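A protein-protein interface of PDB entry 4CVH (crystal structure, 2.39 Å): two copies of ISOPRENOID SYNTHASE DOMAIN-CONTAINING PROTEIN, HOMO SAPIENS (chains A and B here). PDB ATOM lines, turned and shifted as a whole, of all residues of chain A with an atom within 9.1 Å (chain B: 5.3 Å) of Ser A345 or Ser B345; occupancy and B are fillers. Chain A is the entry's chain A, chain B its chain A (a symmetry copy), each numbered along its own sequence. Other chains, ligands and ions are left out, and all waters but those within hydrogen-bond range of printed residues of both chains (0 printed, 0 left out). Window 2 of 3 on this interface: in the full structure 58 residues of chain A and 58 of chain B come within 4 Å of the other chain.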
ATOM      1  N   SER A 306       9.076 -20.218  10.657  1.00  0.00           N
ATOM      2  CA  SER A 306       7.682 -20.610  10.452  1.00  0.00           C
ATOM      3  C   SER A 306       7.463 -22.008  11.053  1.00  0.00           C
ATOM      4  O   SER A 306       6.540 -22.727  10.657  1.00  0.00           O
ATOM      5  CB  SER A 306       7.355 -20.600   8.953  1.00  0.00           C
ATOM      6  OG  SER A 306       5.961 -20.489   8.717  1.00  0.00           O
ATOM      7  N   PHE A 339       1.799 -10.388   8.438  1.00  0.00           N
ATOM      8  CA  PHE A 339       0.599 -10.634   7.630  1.00  0.00           C
ATOM      9  C   PHE A 339      -0.475  -9.584   7.924  1.00  0.00           C
ATOM     10  O   PHE A 339      -0.524  -9.046   9.032  1.00  0.00           O
ATOM     11  CB  PHE A 339       0.043 -12.060   7.843  1.00  0.00           C
ATOM     12  CG  PHE A 339      -0.560 -12.317   9.218  1.00  0.00           C
ATOM     13  CD1 PHE A 339       0.224 -12.777  10.269  1.00  0.00           C
ATOM     14  CD2 PHE A 339      -1.925 -12.154   9.438  1.00  0.00           C
ATOM     15  CE1 PHE A 339      -0.333 -13.031  11.515  1.00  0.00           C
ATOM     16  CE2 PHE A 339      -2.488 -12.407  10.683  1.00  0.00           C
ATOM     17  CZ  PHE A 339      -1.688 -12.846  11.721  1.00  0.00           C
ATOM     18  N   LEU A 341      -4.352  -9.828   7.246  1.00  0.00           N
ATOM     19  CA  LEU A 341      -5.450 -10.547   7.913  1.00  0.00           C
ATOM     20  C   LEU A 341      -5.184 -12.049   8.011  1.00  0.00           C
ATOM     21  O   LEU A 341      -5.425 -12.660   9.058  1.00  0.00           O
ATOM     22  CB  LEU A 341      -6.785 -10.305   7.195  1.00  0.00           C
ATOM     23  CG  LEU A 341      -7.608  -9.090   7.636  1.00  0.00           C
ATOM     24  CD1 LEU A 341      -8.807  -8.927   6.715  1.00  0.00           C
ATOM     25  CD2 LEU A 341      -8.071  -9.198   9.084  1.00  0.00           C
ATOM     26  N   VAL A 342      -4.700 -12.633   6.916  1.00  0.00           N
ATOM     27  CA  VAL A 342      -4.339 -14.050   6.872  1.00  0.00           C
ATOM     28  C   VAL A 342      -2.879 -14.171   6.438  1.00  0.00           C
ATOM     29  O   VAL A 342      -2.442 -13.457   5.535  1.00  0.00           O
ATOM     30  CB  VAL A 342      -5.256 -14.855   5.909  1.00  0.00           C
ATOM     31  CG1 VAL A 342      -5.188 -14.329   4.474  1.00  0.00           C
ATOM     32  CG2 VAL A 342      -4.911 -16.339   5.940  1.00  0.00           C
ATOM     33  N   PRO A 343      -2.113 -15.063   7.090  1.00  0.00           N
ATOM     34  CA  PRO A 343      -0.742 -15.281   6.623  1.00  0.00           C
ATOM     35  C   PRO A 343      -0.705 -16.096   5.328  1.00  0.00           C
ATOM     36  O   PRO A 343      -1.644 -16.851   5.058  1.00  0.00           O
ATOM     37  CB  PRO A 343      -0.083 -16.035   7.785  1.00  0.00           C
ATOM     38  CG  PRO A 343      -1.204 -16.679   8.513  1.00  0.00           C
ATOM     39  CD  PRO A 343      -2.401 -15.793   8.339  1.00  0.00           C
ATOM     40  N   PRO A 344       0.372 -15.947   4.526  1.00  0.00           N
ATOM     41  CA  PRO A 344       0.463 -16.662   3.248  1.00  0.00           C
ATOM     42  C   PRO A 344       0.202 -18.157   3.400  1.00  0.00           C
ATOM     43  O   PRO A 344       0.532 -18.740   4.434  1.00  0.00           O
ATOM     44  CB  PRO A 344       1.908 -16.406   2.787  1.00  0.00           C
ATOM     45  CG  PRO A 344       2.624 -15.833   3.969  1.00  0.00           C
ATOM     46  CD  PRO A 344       1.580 -15.147   4.791  1.00  0.00           C
ATOM     47  N   SER A 345      -0.388 -18.755   2.369  1.00  0.00           N
ATOM     48  CA  SER A 345      -0.825 -20.150   2.408  1.00  0.00           C
ATOM     49  C   SER A 345       0.284 -21.128   2.796  1.00  0.00           C
ATOM     50  O   SER A 345       0.066 -21.990   3.646  1.00  0.00           O
ATOM     51  CB  SER A 345      -1.423 -20.562   1.057  1.00  0.00           C
ATOM     52  OG  SER A 345      -2.612 -19.840   0.780  1.00  0.00           O
ATOM     53  N   GLN A 346       1.461 -20.997   2.183  1.00  0.00           N
ATOM     54  CA  GLN A 346       2.555 -21.959   2.409  1.00  0.00           C
ATOM     55  C   GLN A 346       3.111 -21.920   3.845  1.00  0.00           C
ATOM     56  O   GLN A 346       3.483 -22.963   4.393  1.00  0.00           O
ATOM     57  CB  GLN A 346       3.680 -21.798   1.365  1.00  0.00           C
ATOM     58  CG  GLN A 346       4.763 -20.767   1.680  1.00  0.00           C
ATOM     59  CD  GLN A 346       4.239 -19.340   1.763  1.00  0.00           C
ATOM     60  OE1 GLN A 346       3.330 -18.955   1.020  1.00  0.00           O
ATOM     61  NE2 GLN A 346       4.816 -18.543   2.669  1.00  0.00           N
ATOM     62  N   LYS A 347       3.156 -20.726   4.447  1.00  0.00           N
ATOM     63  CA  LYS A 347       3.605 -20.562   5.832  1.00  0.00           C
ATOM     64  C   LYS A 347       2.571 -21.167   6.777  1.00  0.00           C
ATOM     65  O   LYS A 347       2.924 -21.855   7.739  1.00  0.00           O
ATOM     66  CB  LYS A 347       3.810 -19.083   6.171  1.00  0.00           C
ATOM     67  N   MET A 348       1.295 -20.916   6.478  1.00  0.00           N
ATOM     68  CA  MET A 348       0.184 -21.500   7.223  1.00  0.00           C
ATOM     69  C   MET A 348       0.224 -23.027   7.188  1.00  0.00           C
ATOM     70  O   MET A 348      -0.057 -23.666   8.193  1.00  0.00           O
ATOM     71  CB  MET A 348      -1.161 -20.988   6.692  1.00  0.00           C
ATOM     72  CG  MET A 348      -2.327 -21.221   7.646  1.00  0.00           C
ATOM     73  SD  MET A 348      -2.441 -20.019   8.986  1.00  0.00           S
ATOM     74  CE  MET A 348      -3.905 -19.099   8.506  1.00  0.00           C
ATOM     75  N   GLU A 349       0.588 -23.609   6.046  1.00  0.00           N
ATOM     76  CA  GLU A 349       0.766 -25.065   5.941  1.00  0.00           C
ATOM     77  C   GLU A 349       1.787 -25.613   6.953  1.00  0.00           C
ATOM     78  O   GLU A 349       1.611 -26.719   7.472  1.00  0.00           O
ATOM     79  CB  GLU A 349       1.198 -25.470   4.518  1.00  0.00           C
ATOM     80  CG  GLU A 349       0.105 -25.397   3.458  1.00  0.00           C
ATOM     81  CD  GLU A 349       0.604 -25.780   2.071  1.00  0.00           C
ATOM     82  OE1 GLU A 349       1.262 -26.838   1.941  1.00  0.00           O
ATOM     83  OE2 GLU A 349       0.338 -25.026   1.108  1.00  0.00           O
ATOM     84  N   ASN A 350       2.856 -24.855   7.206  1.00  0.00           N
ATOM     85  CA  ASN A 350       3.915 -25.281   8.132  1.00  0.00           C
ATOM     86  C   ASN A 350       3.434 -25.219   9.573  1.00  0.00           C
ATOM     87  O   ASN A 350       3.697 -26.118  10.363  1.00  0.00           O
ATOM     88  CB  ASN A 350       5.163 -24.401   7.999  1.00  0.00           C
ATOM     89  CG  ASN A 350       5.697 -24.331   6.572  1.00  0.00           C
ATOM     90  OD1 ASN A 350       5.498 -25.240   5.763  1.00  0.00           O
ATOM     91  ND2 ASN A 350       6.384 -23.237   6.259  1.00  0.00           N
ATOM     92  N   LEU A 351       2.727 -24.136   9.900  1.00  0.00           N
ATOM     93  CA  LEU A 351       2.173 -23.930  11.231  1.00  0.00           C
ATOM     94  C   LEU A 351       1.177 -25.017  11.642  1.00  0.00           C
ATOM     95  O   LEU A 351       0.984 -25.263  12.822  1.00  0.00           O
ATOM     96  CB  LEU A 351       1.488 -22.564  11.308  1.00  0.00           C
ATOM     97  CG  LEU A 351       2.377 -21.329  11.132  1.00  0.00           C
ATOM     98  CD1 LEU A 351       1.529 -20.087  10.900  1.00  0.00           C
ATOM     99  CD2 LEU A 351       3.298 -21.141  12.323  1.00  0.00           C
ATOM    100  N   MET A 352       0.556 -25.679  10.675  1.00  0.00           N
ATOM    101  CA  MET A 352      -0.428 -26.714  10.977  1.00  0.00           C
ATOM    102  C   MET A 352       0.165 -28.022  11.508  1.00  0.00           C
ATOM    103  O   MET A 352      -0.581 -28.918  11.899  1.00  0.00           O
ATOM    104  CB  MET A 352      -1.293 -26.977   9.756  1.00  0.00           C
ATOM    105  CG  MET A 352      -2.107 -25.764   9.326  1.00  0.00           C
ATOM    106  SD  MET A 352      -3.482 -25.365  10.420  1.00  0.00           S
ATOM    107  CE  MET A 352      -4.639 -26.657   9.953  1.00  0.00           C
ATOM    108  N   LEU A 408      -4.776 -23.224  15.782  1.00  0.00           N
ATOM    109  CA  LEU A 408      -4.011 -21.998  15.570  1.00  0.00           C
ATOM    110  C   LEU A 408      -4.906 -20.809  15.745  1.00  0.00           C
ATOM    111  O   LEU A 408      -5.710 -20.507  14.868  1.00  0.00           O
ATOM    112  CB  LEU A 408      -3.436 -21.944  14.160  1.00  0.00           C
ATOM    113  CG  LEU A 408      -2.181 -22.758  13.905  1.00  0.00           C
ATOM    114  CD1 LEU A 408      -1.888 -22.729  12.416  1.00  0.00           C
ATOM    115  CD2 LEU A 408      -1.002 -22.209  14.691  1.00  0.00           C
ATOM    116  N   VAL B 342      -4.760 -26.261   4.640  1.00  0.00           N
ATOM    117  CA  VAL B 342      -5.158 -24.861   4.785  1.00  0.00           C
ATOM    118  C   VAL B 342      -6.020 -24.470   3.585  1.00  0.00           C
ATOM    119  O   VAL B 342      -5.712 -24.848   2.454  1.00  0.00           O
ATOM    120  CB  VAL B 342      -3.929 -23.915   4.897  1.00  0.00           C
ATOM    121  CG1 VAL B 342      -3.022 -24.001   3.669  1.00  0.00           C
ATOM    122  CG2 VAL B 342      -4.368 -22.474   5.124  1.00  0.00           C
ATOM    123  N   PRO B 343      -7.113 -23.725   3.826  1.00  0.00           N
ATOM    124  CA  PRO B 343      -7.894 -23.242   2.686  1.00  0.00           C
ATOM    125  C   PRO B 343      -7.191 -22.092   1.960  1.00  0.00           C
ATOM    126  O   PRO B 343      -6.379 -21.395   2.573  1.00  0.00           O
ATOM    127  CB  PRO B 343      -9.214 -22.785   3.324  1.00  0.00           C
ATOM    128  CG  PRO B 343      -8.878 -22.496   4.741  1.00  0.00           C
ATOM    129  CD  PRO B 343      -7.755 -23.416   5.117  1.00  0.00           C
ATOM    130  N   PRO B 344      -7.498 -21.894   0.660  1.00  0.00           N
ATOM    131  CA  PRO B 344      -6.837 -20.839  -0.117  1.00  0.00           C
ATOM    132  C   PRO B 344      -6.888 -19.486   0.583  1.00  0.00           C
ATOM    133  O   PRO B 344      -7.855 -19.190   1.288  1.00  0.00           O
ATOM    134  CB  PRO B 344      -7.631 -20.802  -1.434  1.00  0.00           C
ATOM    135  CG  PRO B 344      -8.867 -21.609  -1.196  1.00  0.00           C
ATOM    136  CD  PRO B 344      -8.511 -22.606  -0.138  1.00  0.00           C
ATOM    137  N   SER B 345      -5.847 -18.683   0.382  1.00  0.00           N
ATOM    138  CA  SER B 345      -5.681 -17.411   1.083  1.00  0.00           C
ATOM    139  C   SER B 345      -6.880 -16.474   0.942  1.00  0.00           C
ATOM    140  O   SER B 345      -7.338 -15.917   1.938  1.00  0.00           O
ATOM    141  CB  SER B 345      -4.412 -16.696   0.601  1.00  0.00           C
ATOM    142  OG  SER B 345      -3.247 -17.429   0.946  1.00  0.00           O
ATOM    143  N   GLN B 346      -7.385 -16.302  -0.281  1.00  0.00           N
ATOM    144  CA  GLN B 346      -8.468 -15.335  -0.534  1.00  0.00           C
ATOM    145  C   GLN B 346      -9.799 -15.723   0.141  1.00  0.00           C
ATOM    146  O   GLN B 346     -10.539 -14.846   0.599  1.00  0.00           O
ATOM    147  CB  GLN B 346      -8.659 -15.074  -2.043  1.00  0.00           C
ATOM    148  CG  GLN B 346      -9.583 -16.033  -2.791  1.00  0.00           C
ATOM    149  CD  GLN B 346      -9.083 -17.471  -2.807  1.00  0.00           C
ATOM    150  OE1 GLN B 346      -7.875 -17.721  -2.881  1.00  0.00           O
ATOM    151  NE2 GLN B 346     -10.015 -18.428  -2.744  1.00  0.00           N
ATOM    152  N   LYS B 347     -10.088 -17.028   0.208  1.00  0.00           N
ATOM    153  CA  LYS B 347     -11.289 -17.531   0.877  1.00  0.00           C
ATOM    154  C   LYS B 347     -11.153 -17.332   2.384  1.00  0.00           C
ATOM    155  O   LYS B 347     -12.104 -16.912   3.051  1.00  0.00           O
ATOM    156  CB  LYS B 347     -11.507 -19.016   0.572  1.00  0.00           C
ATOM    157  N   MET B 348      -9.958 -17.618   2.901  1.00  0.00           N
ATOM    158  CA  MET B 348      -9.634 -17.390   4.306  1.00  0.00           C
ATOM    159  C   MET B 348      -9.802 -15.921   4.691  1.00  0.00           C
ATOM    160  O   MET B 348     -10.287 -15.627   5.775  1.00  0.00           O
ATOM    161  CB  MET B 348      -8.212 -17.867   4.625  1.00  0.00           C
ATOM    162  CG  MET B 348      -7.941 -18.038   6.115  1.00  0.00           C
ATOM    163  SD  MET B 348      -8.573 -19.577   6.813  1.00  0.00           S
ATOM    164  CE  MET B 348      -7.048 -20.469   7.128  1.00  0.00           C
ATOM    165  N   GLU B 349      -9.422 -15.003   3.803  1.00  0.00           N
ATOM    166  CA  GLU B 349      -9.645 -13.568   4.029  1.00  0.00           C
ATOM    167  C   GLU B 349     -11.125 -13.226   4.271  1.00  0.00           C
ATOM    168  O   GLU B 349     -11.433 -12.339   5.072  1.00  0.00           O
ATOM    169  CB  GLU B 349      -9.122 -12.731   2.844  1.00  0.00           C
ATOM    170  CG  GLU B 349      -7.606 -12.613   2.748  1.00  0.00           C
ATOM    171  CD  GLU B 349      -7.154 -11.801   1.541  1.00  0.00           C
ATOM    172  OE1 GLU B 349      -7.688 -10.687   1.333  1.00  0.00           O
ATOM    173  OE2 GLU B 349      -6.263 -12.273   0.799  1.00  0.00           O
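Among the printed residues, merely in contact across the chains: Val A342 with Ser B345, Val A342 with Met B348, Val A342 with Glu B349, Ser A345 with Val B342, Met A348 with Val B342, Met A348 with Met B348 and Glu A349 with Val B342.
Of chain B, only Val B342 and Ser B345 come within 4 Å of Ser A345. Ser B345 touches just these residues of chain A: Val A342 and Ser A345. Of the printed residues of chain A, Glu B349 touches Val A342 (3.4 Å). Printed residues of chain B within 4 Å of Glu A349: Val B342 (3.4 Å). The nearest residue of chain B that does not touch Ser A345 is Pro B344 (4.3 Å). The nearest residue of chain A that does not touch Ser B345 is Pro A344 (4.3 Å).
The side-chain hydroxyl (OG) of Ser A345 lies within hydrogen-bond range of the side-chain hydroxyl (OG) of Ser B345, 2.5 Å away.
Printed residues of chain B that touch a printed residue of chain A: Val B342, Ser B345, Met B348 and Glu B349. Hydrophobic or aromatic side chains of chain B that line the printed part of chain A: Val B342 and Met B348. Of the 15 printed residues of chain A, 4 touch a printed residue of chain B. Among the printed residues, 8 pairs touch across the chains. Among the printed residues, no Asp or Glu carboxylate lies within 4 Å of a Lys or Arg side-chain nitrogen of the other chain.
Val A342 touches Ser B345, and with the chains exchanged Ser A345 touches Val B342. Val A342 touches Met B348, and with the chains exchanged Met A348 touches Val B342. Val A342 touches Glu B349, and with the chains exchanged Glu A349 touches Val B342. Met B348 touches its own counterpart, Met A348. Positions printed for both chains: 342, 343, 344, 345, 346, 347, 348 and 349. Of the 8 pairs that touch across the chains among the printed residues, 8 have their exchanged pair printed and touching as well.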
